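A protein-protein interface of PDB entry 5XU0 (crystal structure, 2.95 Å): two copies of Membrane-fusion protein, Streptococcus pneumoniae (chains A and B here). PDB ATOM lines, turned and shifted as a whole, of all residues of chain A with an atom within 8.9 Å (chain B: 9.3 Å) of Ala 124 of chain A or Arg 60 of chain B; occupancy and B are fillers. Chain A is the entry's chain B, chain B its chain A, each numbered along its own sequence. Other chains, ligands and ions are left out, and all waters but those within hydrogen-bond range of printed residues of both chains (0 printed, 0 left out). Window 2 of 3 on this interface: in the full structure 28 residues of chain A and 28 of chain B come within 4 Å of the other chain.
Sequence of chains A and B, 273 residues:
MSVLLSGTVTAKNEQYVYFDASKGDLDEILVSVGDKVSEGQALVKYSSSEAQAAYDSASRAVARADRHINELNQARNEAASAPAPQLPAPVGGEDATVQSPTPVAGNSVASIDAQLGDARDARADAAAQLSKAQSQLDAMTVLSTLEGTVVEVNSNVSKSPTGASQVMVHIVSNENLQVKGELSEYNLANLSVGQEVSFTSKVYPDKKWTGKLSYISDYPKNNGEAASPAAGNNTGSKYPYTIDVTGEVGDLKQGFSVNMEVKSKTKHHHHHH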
ATOM      1  N   ALA A  61       6.814  -9.801  15.624  1.00  0.00           N
ATOM      2  CA  ALA A  61       7.730  -9.446  16.703  1.00  0.00           C
ATOM      3  C   ALA A  61       8.700  -8.359  16.260  1.00  0.00           C
ATOM      4  O   ALA A  61       8.974  -7.416  17.014  1.00  0.00           O
ATOM      5  CB  ALA A  61       8.486 -10.683  17.187  1.00  0.00           C
ATOM      6  N   VAL A  62       9.225  -8.463  15.034  1.00  0.00           N
ATOM      7  CA  VAL A  62      10.109  -7.411  14.533  1.00  0.00           C
ATOM      8  C   VAL A  62       9.330  -6.120  14.311  1.00  0.00           C
ATOM      9  O   VAL A  62       9.850  -5.016  14.524  1.00  0.00           O
ATOM     10  CB  VAL A  62      10.817  -7.869  13.248  1.00  0.00           C
ATOM     11  CG1 VAL A  62      12.027  -6.987  12.970  1.00  0.00           C
ATOM     12  CG2 VAL A  62      11.226  -9.328  13.361  1.00  0.00           C
ATOM     13  N   ALA A  65       8.655  -4.585  17.707  1.00  0.00           N
ATOM     14  CA  ALA A  65       9.933  -4.105  18.225  1.00  0.00           C
ATOM     15  C   ALA A  65      10.329  -2.783  17.579  1.00  0.00           C
ATOM     16  O   ALA A  65      10.739  -1.842  18.274  1.00  0.00           O
ATOM     17  CB  ALA A  65      11.017  -5.160  18.002  1.00  0.00           C
ATOM     18  N   ASP A  66      10.211  -2.694  16.251  1.00  0.00           N
ATOM     19  CA  ASP A  66      10.507  -1.443  15.557  1.00  0.00           C
ATOM     20  C   ASP A  66       9.608  -0.320  16.055  1.00  0.00           C
ATOM     21  O   ASP A  66      10.078   0.790  16.337  1.00  0.00           O
ATOM     22  CB  ASP A  66      10.345  -1.632  14.050  1.00  0.00           C
ATOM     23  CG  ASP A  66      11.477  -2.432  13.438  1.00  0.00           C
ATOM     24  OD1 ASP A  66      12.579  -2.459  14.027  1.00  0.00           O
ATOM     25  OD2 ASP A  66      11.261  -3.034  12.364  1.00  0.00           O
ATOM     26  N   ILE A  69      11.008   0.865  19.426  1.00  0.00           N
ATOM     27  CA  ILE A  69      12.194   1.712  19.308  1.00  0.00           C
ATOM     28  C   ILE A  69      11.810   3.097  18.795  1.00  0.00           C
ATOM     29  O   ILE A  69      12.344   4.118  19.254  1.00  0.00           O
ATOM     30  CB  ILE A  69      13.249   1.039  18.409  1.00  0.00           C
ATOM     31  CG1 ILE A  69      13.894  -0.144  19.140  1.00  0.00           C
ATOM     32  CG2 ILE A  69      14.311   2.042  17.968  1.00  0.00           C
ATOM     33  CD1 ILE A  69      15.205  -0.607  18.535  1.00  0.00           C
ATOM     34  N   GLY A 117      18.193   0.684  25.228  1.00  0.00           N
ATOM     35  CA  GLY A 117      19.059  -0.476  25.334  1.00  0.00           C
ATOM     36  C   GLY A 117      18.309  -1.774  25.551  1.00  0.00           C
ATOM     37  O   GLY A 117      18.807  -2.839  25.173  1.00  0.00           O
ATOM     38  N   ASP A 118      17.116  -1.714  26.146  1.00  0.00           N
ATOM     39  CA  ASP A 118      16.310  -2.913  26.337  1.00  0.00           C
ATOM     40  C   ASP A 118      15.344  -3.184  25.189  1.00  0.00           C
ATOM     41  O   ASP A 118      14.716  -4.246  25.171  1.00  0.00           O
ATOM     42  CB  ASP A 118      15.537  -2.821  27.655  1.00  0.00           C
ATOM     43  CG  ASP A 118      16.406  -3.136  28.860  1.00  0.00           C
ATOM     44  OD1 ASP A 118      17.637  -3.266  28.686  1.00  0.00           O
ATOM     45  OD2 ASP A 118      15.864  -3.255  29.980  1.00  0.00           O
ATOM     46  N   ALA A 119      15.204  -2.260  24.238  1.00  0.00           N
ATOM     47  CA  ALA A 119      14.413  -2.514  23.042  1.00  0.00           C
ATOM     48  C   ALA A 119      15.259  -2.952  21.857  1.00  0.00           C
ATOM     49  O   ALA A 119      14.747  -3.653  20.977  1.00  0.00           O
ATOM     50  CB  ALA A 119      13.607  -1.268  22.655  1.00  0.00           C
ATOM     51  N   ARG A 120      16.533  -2.552  21.809  1.00  0.00           N
ATOM     52  CA  ARG A 120      17.435  -3.123  20.814  1.00  0.00           C
ATOM     53  C   ARG A 120      17.675  -4.603  21.084  1.00  0.00           C
ATOM     54  O   ARG A 120      17.767  -5.409  20.150  1.00  0.00           O
ATOM     55  CB  ARG A 120      18.758  -2.358  20.795  1.00  0.00           C
ATOM     56  CG  ARG A 120      18.613  -0.852  20.674  1.00  0.00           C
ATOM     57  CD  ARG A 120      19.972  -0.188  20.542  1.00  0.00           C
ATOM     58  NE  ARG A 120      20.056   1.036  21.338  1.00  0.00           N
ATOM     59  CZ  ARG A 120      21.022   1.286  22.215  1.00  0.00           C
ATOM     60  NH1 ARG A 120      21.990   0.400  22.409  1.00  0.00           N
ATOM     61  NH2 ARG A 120      21.020   2.422  22.897  1.00  0.00           N
ATOM     62  N   ASP A 121      17.779  -4.979  22.359  1.00  0.00           N
ATOM     63  CA  ASP A 121      17.854  -6.393  22.706  1.00  0.00           C
ATOM     64  C   ASP A 121      16.599  -7.128  22.257  1.00  0.00           C
ATOM     65  O   ASP A 121      16.677  -8.214  21.670  1.00  0.00           O
ATOM     66  CB  ASP A 121      18.061  -6.551  24.214  1.00  0.00           C
ATOM     67  CG  ASP A 121      19.500  -6.326  24.631  1.00  0.00           C
ATOM     68  OD1 ASP A 121      20.326  -5.972  23.762  1.00  0.00           O
ATOM     69  OD2 ASP A 121      19.804  -6.507  25.829  1.00  0.00           O
ATOM     70  N   ALA A 122      15.428  -6.539  22.517  1.00  0.00           N
ATOM     71  CA  ALA A 122      14.173  -7.158  22.102  1.00  0.00           C
ATOM     72  C   ALA A 122      14.113  -7.333  20.589  1.00  0.00           C
ATOM     73  O   ALA A 122      13.639  -8.365  20.096  1.00  0.00           O
ATOM     74  CB  ALA A 122      12.992  -6.326  22.597  1.00  0.00           C
ATOM     75  N   ARG A 123      14.592  -6.341  19.834  1.00  0.00           N
ATOM     76  CA  ARG A 123      14.581  -6.471  18.380  1.00  0.00           C
ATOM     77  C   ARG A 123      15.587  -7.513  17.901  1.00  0.00           C
ATOM     78  O   ARG A 123      15.346  -8.182  16.888  1.00  0.00           O
ATOM     79  CB  ARG A 123      14.842  -5.114  17.715  1.00  0.00           C
ATOM     80  CG  ARG A 123      16.310  -4.745  17.559  1.00  0.00           C
ATOM     81  CD  ARG A 123      16.556  -3.897  16.324  1.00  0.00           C
ATOM     82  NE  ARG A 123      15.774  -4.352  15.179  1.00  0.00           N
ATOM     83  CZ  ARG A 123      16.111  -5.377  14.402  1.00  0.00           C
ATOM     84  NH1 ARG A 123      17.220  -6.064  14.649  1.00  0.00           N
ATOM     85  NH2 ARG A 123      15.340  -5.717  13.378  1.00  0.00           N
ATOM     86  N   ALA A 124      16.707  -7.675  18.612  1.00  0.00           N
ATOM     87  CA  ALA A 124      17.656  -8.720  18.241  1.00  0.00           C
ATOM     88  C   ALA A 124      17.068 -10.103  18.497  1.00  0.00           C
ATOM     89  O   ALA A 124      17.208 -11.012  17.666  1.00  0.00           O
ATOM     90  CB  ALA A 124      18.967  -8.537  19.003  1.00  0.00           C
ATOM     91  N   ASP A 125      16.401 -10.278  19.640  1.00  0.00           N
ATOM     92  CA  ASP A 125      15.696 -11.527  19.902  1.00  0.00           C
ATOM     93  C   ASP A 125      14.633 -11.784  18.842  1.00  0.00           C
ATOM     94  O   ASP A 125      14.445 -12.925  18.403  1.00  0.00           O
ATOM     95  CB  ASP A 125      15.063 -11.493  21.295  1.00  0.00           C
ATOM     96  CG  ASP A 125      16.096 -11.471  22.407  1.00  0.00           C
ATOM     97  OD1 ASP A 125      17.239 -11.921  22.179  1.00  0.00           O
ATOM     98  OD2 ASP A 125      15.761 -11.002  23.514  1.00  0.00           O
ATOM     99  N   ALA A 126      13.927 -10.735  18.416  1.00  0.00           N
ATOM    100  CA  ALA A 126      12.903 -10.903  17.391  1.00  0.00           C
ATOM    101  C   ALA A 126      13.517 -11.324  16.061  1.00  0.00           C
ATOM    102  O   ALA A 126      12.946 -12.148  15.339  1.00  0.00           O
ATOM    103  CB  ALA A 126      12.101  -9.612  17.230  1.00  0.00           C
ATOM    104  N   ALA A 127      14.683 -10.769  15.722  1.00  0.00           N
ATOM    105  CA  ALA A 127      15.358 -11.167  14.491  1.00  0.00           C
ATOM    106  C   ALA A 127      15.787 -12.627  14.551  1.00  0.00           C
ATOM    107  O   ALA A 127      15.531 -13.404  13.621  1.00  0.00           O
ATOM    108  CB  ALA A 127      16.563 -10.260  14.237  1.00  0.00           C
ATOM    109  N   ALA A 128      16.441 -13.020  15.648  1.00  0.00           N
ATOM    110  CA  ALA A 128      16.869 -14.408  15.796  1.00  0.00           C
ATOM    111  C   ALA A 128      15.682 -15.360  15.714  1.00  0.00           C
ATOM    112  O   ALA A 128      15.735 -16.382  15.018  1.00  0.00           O
ATOM    113  CB  ALA A 128      17.618 -14.586  17.118  1.00  0.00           C
ATOM    114  N   GLN A 129      14.595 -15.035  16.419  1.00  0.00           N
ATOM    115  CA  GLN A 129      13.381 -15.840  16.338  1.00  0.00           C
ATOM    116  C   GLN A 129      12.883 -15.934  14.900  1.00  0.00           C
ATOM    117  O   GLN A 129      12.476 -17.012  14.439  1.00  0.00           O
ATOM    118  CB  GLN A 129      12.305 -15.244  17.250  1.00  0.00           C
ATOM    119  CG  GLN A 129      10.895 -15.768  17.013  1.00  0.00           C
ATOM    120  CD  GLN A 129       9.863 -15.102  17.909  1.00  0.00           C
ATOM    121  OE1 GLN A 129      10.210 -14.391  18.856  1.00  0.00           O
ATOM    122  NE2 GLN A 129       8.587 -15.335  17.617  1.00  0.00           N
ATOM    123  N   LEU A 130      12.938 -14.818  14.168  1.00  0.00           N
ATOM    124  CA  LEU A 130      12.487 -14.810  12.781  1.00  0.00           C
ATOM    125  C   LEU A 130      13.292 -15.787  11.937  1.00  0.00           C
ATOM    126  O   LEU A 130      12.723 -16.637  11.245  1.00  0.00           O
ATOM    127  CB  LEU A 130      12.581 -13.400  12.200  1.00  0.00           C
ATOM    128  CG  LEU A 130      12.268 -13.319  10.703  1.00  0.00           C
ATOM    129  CD1 LEU A 130      10.772 -13.469  10.452  1.00  0.00           C
ATOM    130  CD2 LEU A 130      12.798 -12.026  10.100  1.00  0.00           C
ATOM    131  N   SER A 131      14.624 -15.684  11.982  1.00  0.00           N
ATOM    132  CA  SER A 131      15.444 -16.578  11.169  1.00  0.00           C
ATOM    133  C   SER A 131      15.288 -18.032  11.600  1.00  0.00           C
ATOM    134  O   SER A 131      15.352 -18.936  10.755  1.00  0.00           O
ATOM    135  CB  SER A 131      16.911 -16.153  11.225  1.00  0.00           C
ATOM    136  OG  SER A 131      17.314 -15.876  12.554  1.00  0.00           O
ATOM    137  N   GLN B  52      24.585 -20.633  17.830  1.00  0.00           N
ATOM    138  CA  GLN B  52      25.091 -19.270  17.691  1.00  0.00           C
ATOM    139  C   GLN B  52      24.052 -18.249  18.137  1.00  0.00           C
ATOM    140  O   GLN B  52      24.395 -17.214  18.722  1.00  0.00           O
ATOM    141  CB  GLN B  52      25.513 -19.015  16.243  1.00  0.00           C
ATOM    142  CG  GLN B  52      26.140 -17.654  16.011  1.00  0.00           C
ATOM    143  CD  GLN B  52      27.500 -17.517  16.669  1.00  0.00           C
ATOM    144  OE1 GLN B  52      28.437 -18.247  16.346  1.00  0.00           O
ATOM    145  NE2 GLN B  52      27.613 -16.579  17.602  1.00  0.00           N
ATOM    146  N   ALA B  53      22.774 -18.529  17.876  1.00  0.00           N
ATOM    147  CA  ALA B  53      21.713 -17.624  18.303  1.00  0.00           C
ATOM    148  C   ALA B  53      21.589 -17.602  19.823  1.00  0.00           C
ATOM    149  O   ALA B  53      21.493 -16.528  20.433  1.00  0.00           O
ATOM    150  CB  ALA B  53      20.388 -18.025  17.655  1.00  0.00           C
ATOM    151  N   ALA B  54      21.589 -18.781  20.453  1.00  0.00           N
ATOM    152  CA  ALA B  54      21.563 -18.837  21.911  1.00  0.00           C
ATOM    153  C   ALA B  54      22.779 -18.140  22.508  1.00  0.00           C
ATOM    154  O   ALA B  54      22.684 -17.487  23.554  1.00  0.00           O
ATOM    155  CB  ALA B  54      21.490 -20.289  22.381  1.00  0.00           C
ATOM    156  N   TYR B  55      23.931 -18.264  21.847  1.00  0.00           N
ATOM    157  CA  TYR B  55      25.136 -17.577  22.300  1.00  0.00           C
ATOM    158  C   TYR B  55      24.949 -16.065  22.269  1.00  0.00           C
ATOM    159  O   TYR B  55      25.170 -15.373  23.273  1.00  0.00           O
ATOM    160  CB  TYR B  55      26.322 -17.995  21.430  1.00  0.00           C
ATOM    161  CG  TYR B  55      27.616 -17.310  21.798  1.00  0.00           C
ATOM    162  CD1 TYR B  55      28.488 -17.886  22.710  1.00  0.00           C
ATOM    163  CD2 TYR B  55      27.964 -16.088  21.237  1.00  0.00           C
ATOM    164  CE1 TYR B  55      29.671 -17.264  23.054  1.00  0.00           C
ATOM    165  CE2 TYR B  55      29.143 -15.458  21.576  1.00  0.00           C
ATOM    166  CZ  TYR B  55      29.994 -16.051  22.484  1.00  0.00           C
ATOM    167  OH  TYR B  55      31.173 -15.432  22.825  1.00  0.00           O
ATOM    168  N   ASP B  56      24.561 -15.532  21.106  1.00  0.00           N
ATOM    169  CA  ASP B  56      24.332 -14.097  20.976  1.00  0.00           C
ATOM    170  C   ASP B  56      23.344 -13.604  22.026  1.00  0.00           C
ATOM    171  O   ASP B  56      23.583 -12.595  22.699  1.00  0.00           O
ATOM    172  CB  ASP B  56      23.824 -13.772  19.569  1.00  0.00           C
ATOM    173  CG  ASP B  56      24.864 -14.036  18.498  1.00  0.00           C
ATOM    174  OD1 ASP B  56      24.503 -14.599  17.442  1.00  0.00           O
ATOM    175  OD2 ASP B  56      26.043 -13.684  18.713  1.00  0.00           O
ATOM    176  N   SER B  57      22.228 -14.321  22.183  1.00  0.00           N
ATOM    177  CA  SER B  57      21.254 -13.959  23.206  1.00  0.00           C
ATOM    178  C   SER B  57      21.895 -13.939  24.590  1.00  0.00           C
ATOM    179  O   SER B  57      21.569 -13.084  25.425  1.00  0.00           O
ATOM    180  CB  SER B  57      20.077 -14.932  23.164  1.00  0.00           C
ATOM    181  OG  SER B  57      18.982 -14.462  23.930  1.00  0.00           O
ATOM    182  N   ALA B  58      22.832 -14.857  24.843  1.00  0.00           N
ATOM    183  CA  ALA B  58      23.499 -14.889  26.141  1.00  0.00           C
ATOM    184  C   ALA B  58      24.372 -13.656  26.356  1.00  0.00           C
ATOM    185  O   ALA B  58      24.336 -13.047  27.437  1.00  0.00           O
ATOM    186  CB  ALA B  58      24.322 -16.169  26.272  1.00  0.00           C
ATOM    187  N   SER B  59      25.150 -13.265  25.339  1.00  0.00           N
ATOM    188  CA  SER B  59      26.010 -12.094  25.495  1.00  0.00           C
ATOM    189  C   SER B  59      25.202 -10.804  25.591  1.00  0.00           C
ATOM    190  O   SER B  59      25.611  -9.863  26.282  1.00  0.00           O
ATOM    191  CB  SER B  59      27.005 -12.013  24.345  1.00  0.00           C
ATOM    192  OG  SER B  59      26.365 -11.708  23.126  1.00  0.00           O
ATOM    193  N   ARG B  60      24.061 -10.732  24.906  1.00  0.00           N
ATOM    194  CA  ARG B  60      23.171  -9.592  25.093  1.00  0.00           C
ATOM    195  C   ARG B  60      22.583  -9.585  26.497  1.00  0.00           C
ATOM    196  O   ARG B  60      22.374  -8.514  27.078  1.00  0.00           O
ATOM    197  CB  ARG B  60      22.065  -9.603  24.036  1.00  0.00           C
ATOM    198  CG  ARG B  60      22.534  -9.155  22.669  1.00  0.00           C
ATOM    199  CD  ARG B  60      21.362  -8.807  21.772  1.00  0.00           C
ATOM    200  NE  ARG B  60      20.415  -9.911  21.660  1.00  0.00           N
ATOM    201  CZ  ARG B  60      20.600 -10.979  20.891  1.00  0.00           C
ATOM    202  NH1 ARG B  60      21.703 -11.093  20.163  1.00  0.00           N
ATOM    203  NH2 ARG B  60      19.682 -11.935  20.852  1.00  0.00           N
ATOM    204  N   ALA B  61      22.313 -10.769  27.060  1.00  0.00           N
ATOM    205  CA  ALA B  61      21.855 -10.833  28.445  1.00  0.00           C
ATOM    206  C   ALA B  61      22.923 -10.315  29.402  1.00  0.00           C
ATOM    207  O   ALA B  61      22.618  -9.579  30.352  1.00  0.00           O
ATOM    208  CB  ALA B  61      21.457 -12.263  28.801  1.00  0.00           C
ATOM    209  N   VAL B  62      24.187 -10.680  29.163  1.00  0.00           N
ATOM    210  CA  VAL B  62      25.277 -10.183  30.001  1.00  0.00           C
ATOM    211  C   VAL B  62      25.377  -8.665  29.901  1.00  0.00           C
ATOM    212  O   VAL B  62      25.400  -7.954  30.917  1.00  0.00           O
ATOM    213  CB  VAL B  62      26.606 -10.859  29.612  1.00  0.00           C
ATOM    214  CG1 VAL B  62      27.781 -10.095  30.204  1.00  0.00           C
ATOM    215  CG2 VAL B  62      26.619 -12.311  30.068  1.00  0.00           C
ATOM    216  N   ALA B  63      25.431  -8.146  28.670  1.00  0.00           N
ATOM    217  CA  ALA B  63      25.565  -6.704  28.480  1.00  0.00           C
ATOM    218  C   ALA B  63      24.403  -5.948  29.117  1.00  0.00           C
ATOM    219  O   ALA B  63      24.598  -4.883  29.720  1.00  0.00           O
ATOM    220  CB  ALA B  63      25.665  -6.384  26.989  1.00  0.00           C
ATOM    221  N   ARG B  64      23.188  -6.490  29.002  1.00  0.00           N
ATOM    222  CA  ARG B  64      22.032  -5.859  29.630  1.00  0.00           C
ATOM    223  C   ARG B  64      22.151  -5.886  31.148  1.00  0.00           C
ATOM    224  O   ARG B  64      21.744  -4.935  31.827  1.00  0.00           O
ATOM    225  CB  ARG B  64      20.750  -6.551  29.170  1.00  0.00           C
ATOM    226  CG  ARG B  64      19.501  -6.164  29.945  1.00  0.00           C
ATOM    227  CD  ARG B  64      18.295  -6.915  29.417  1.00  0.00           C
ATOM    228  NE  ARG B  64      18.608  -8.323  29.192  1.00  0.00           N
ATOM    229  CZ  ARG B  64      18.081  -9.062  28.221  1.00  0.00           C
ATOM    230  NH1 ARG B  64      17.209  -8.528  27.375  1.00  0.00           N
ATOM    231  NH2 ARG B  64      18.429 -10.335  28.095  1.00  0.00           N
ATOM    232  N   ALA B  65      22.710  -6.965  31.703  1.00  0.00           N
ATOM    233  CA  ALA B  65      22.964  -6.992  33.139  1.00  0.00           C
ATOM    234  C   ALA B  65      23.931  -5.886  33.547  1.00  0.00           C
ATOM    235  O   ALA B  65      23.706  -5.189  34.546  1.00  0.00           O
ATOM    236  CB  ALA B  65      23.504  -8.362  33.553  1.00  0.00           C
ATOM    237  N   ASP B  66      25.004  -5.696  32.771  1.00  0.00           N
ATOM    238  CA  ASP B  66      25.993  -4.679  33.123  1.00  0.00           C
ATOM    239  C   ASP B  66      25.407  -3.275  33.040  1.00  0.00           C
ATOM    240  O   ASP B  66      25.600  -2.460  33.956  1.00  0.00           O
ATOM    241  CB  ASP B  66      27.220  -4.807  32.222  1.00  0.00           C
ATOM    242  CG  ASP B  66      28.262  -5.744  32.796  1.00  0.00           C
ATOM    243  OD1 ASP B  66      28.013  -6.306  33.882  1.00  0.00           O
ATOM    244  OD2 ASP B  66      29.328  -5.915  32.167  1.00  0.00           O
ATOM    245  N   ARG B  67      24.696  -2.969  31.954  1.00  0.00           N
ATOM    246  CA  ARG B  67      23.976  -1.702  31.889  1.00  0.00           C
ATOM    247  C   ARG B  67      23.085  -1.534  33.114  1.00  0.00           C
ATOM    248  O   ARG B  67      23.263  -0.597  33.903  1.00  0.00           O
ATOM    249  CB  ARG B  67      23.159  -1.622  30.597  1.00  0.00           C
ATOM    250  CG  ARG B  67      24.017  -1.520  29.339  1.00  0.00           C
ATOM    251  CD  ARG B  67      23.201  -1.159  28.105  1.00  0.00           C
ATOM    252  NE  ARG B  67      22.489  -2.310  27.555  1.00  0.00           N
ATOM    253  CZ  ARG B  67      21.197  -2.551  27.760  1.00  0.00           C
ATOM    254  NH1 ARG B  67      20.480  -1.717  28.500  1.00  0.00           N
ATOM    255  NH2 ARG B  67      20.625  -3.622  27.226  1.00  0.00           N
ATOM    256  N   HIS B  68      22.156  -2.474  33.316  1.00  0.00           N
ATOM    257  CA  HIS B  68      21.224  -2.423  34.440  1.00  0.00           C
ATOM    258  C   HIS B  68      21.913  -2.076  35.759  1.00  0.00           C
ATOM    259  O   HIS B  68      21.455  -1.191  36.497  1.00  0.00           O
ATOM    260  CB  HIS B  68      20.487  -3.761  34.549  1.00  0.00           C
ATOM    261  CG  HIS B  68      19.371  -3.915  33.564  1.00  0.00           C
ATOM    262  ND1 HIS B  68      18.367  -4.849  33.713  1.00  0.00           N
ATOM    263  CD2 HIS B  68      19.096  -3.249  32.416  1.00  0.00           C
ATOM    264  CE1 HIS B  68      17.524  -4.754  32.700  1.00  0.00           C
ATOM    265  NE2 HIS B  68      17.944  -3.792  31.899  1.00  0.00           N
ATOM    266  N   ALA B 126      23.903 -14.811  33.985  1.00  0.00           N
ATOM    267  CA  ALA B 126      24.047 -14.659  32.542  1.00  0.00           C
ATOM    268  C   ALA B 126      25.471 -14.949  32.082  1.00  0.00           C
ATOM    269  O   ALA B 126      25.672 -15.428  30.959  1.00  0.00           O
ATOM    270  CB  ALA B 126      23.624 -13.252  32.116  1.00  0.00           C
ATOM    271  N   ALA B 127      26.468 -14.673  32.926  1.00  0.00           N
ATOM    272  CA  ALA B 127      27.850 -14.978  32.563  1.00  0.00           C
ATOM    273  C   ALA B 127      28.058 -16.483  32.425  1.00  0.00           C
ATOM    274  O   ALA B 127      28.530 -16.974  31.385  1.00  0.00           O
ATOM    275  CB  ALA B 127      28.805 -14.391  33.605  1.00  0.00           C
ATOM    276  N   LEU B 130      26.412 -17.807  29.464  1.00  0.00           N
ATOM    277  CA  LEU B 130      27.130 -17.488  28.234  1.00  0.00           C
ATOM    278  C   LEU B 130      28.252 -18.482  27.979  1.00  0.00           C
ATOM    279  O   LEU B 130      28.415 -18.961  26.854  1.00  0.00           O
ATOM    280  CB  LEU B 130      27.691 -16.068  28.268  1.00  0.00           C
ATOM    281  CG  LEU B 130      28.432 -15.807  26.948  1.00  0.00           C
ATOM    282  CD1 LEU B 130      27.587 -15.006  26.002  1.00  0.00           C
ATOM    283  CD2 LEU B 130      29.779 -15.121  27.160  1.00  0.00           C
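The guanidinium group (NH2) of Arg 67 of chain B lies within hydrogen-bond range of the backbone carbonyl oxygen (O) of Gly 117 of chain A, 2.9 Å away.
The guanidinium group of Arg 67 of chain B lies within salt-bridge range of the side-chain carboxylate of Asp 118 of chain A, at 3.2 Å.
NH2 of Arg 60 of chain B lies within salt-bridge range of OD1 of Asp 125 of chain A, at 2.8 Å.
OD2 of Asp 121 of chain A sits close to O of Arg 60 of chain B, at 3.5 Å.
The side-chain carboxylate of Asp 118 of chain A lies within hydrogen-bond range of a ring nitrogen (NE2) of His 68 of chain B.
NH1 of Arg 64 of chain B is in salt-bridge range of OD2 of Asp 121 of chain A (3.6 Å).
The guanidinium group (NH2) of Arg 67 of chain B lies within salt-bridge range of the side-chain carboxylate (OD2) of Asp 121 of chain A, 3.3 Å away.
The backbone carbonyl oxygen (O) of Asp 56 of chain B lies close to the guanidinium group (NH1) of Arg 60 of chain B (3.5 Å).
Asp 118 of chain A touches Arg 64 of chain B (OD1 to CG, 3.7 Å).
CB of Ala 124 of chain A touches NE of Arg 60 of chain B, at 3.3 Å.
Asp 125 of chain A touches Ser 57 of chain B.
Of the printed residues of chain B, Gly 117 of chain A touches Arg 67 (2.9 Å).
Of the printed residues of chain B, Asp 118 of chain A touches Arg 64 (3.7 Å), Arg 67 (3.2 Å) and His 68 (2.9 Å).
Ala 124 of chain A touches one residue of chain B.
Asp 125 of chain A touches just these residues of chain B: Ser 57 (3.5 Å) and Arg 60 (2.8 Å).
Ala 128 of chain A touches none of the printed residues of chain B.
No residue of chain A comes within 4 Å of Ser 59 of chain B.
Printed residues of chain A within 4 Å of Arg 60 of chain B: Asp 121 (3.5 Å), Ala 124 (3.3 Å) and Asp 125 (2.8 Å).
Ala 61 of chain B touches none of the printed residues of chain A.
Of the printed residues of chain A, Arg 67 of chain B touches Gly 117, Asp 118 and Asp 121.
Printed residues of chain A within 4 Å of His 68 of chain B: Asp 118 (2.9 Å).
The nearest residue of chain B that does not touch Ala 124 of chain A is Asp 56 of chain B (7.2 Å).
The nearest printed residue of chain A that does not touch Arg 67 of chain B is Arg 120 of chain A (5.8 Å).
Of the 20 printed residues of chain B, 5 touch a printed residue of chain A.
Printed residues of chain B that touch a printed residue of chain A: Ser 57, Arg 60, Arg 64, Arg 67 and His 68.
Hydrophobic or aromatic side chains of chain B within 4 Å of the printed part of chain A: His 68.
Printed residues of chain A that touch a printed residue of chain B: Gly 117, Asp 118, Asp 121, Ala 124 and Asp 125.
Hydrophobic or aromatic side chains of chain A that line the printed part of chain B: Ala 124.
Among the printed residues, 10 pairs touch across the chains.
Among the printed residues, Asp or Glu carboxylates within 4 Å of a Lys or Arg side-chain nitrogen of the other chain: Asp 118 of chain A with Arg 67 of chain B, Asp 121 of chain A with Arg 64 of chain B, Asp 121 of chain A with Arg 67 of chain B and Asp 125 of chain A with Arg 60 of chain B.
Positions printed for both chains: 61, 62, 65, 66, 126, 127 and 130.
Of the 10 pairs that touch across the chains among the printed residues, none has its exchanged pair printed and touching as well.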
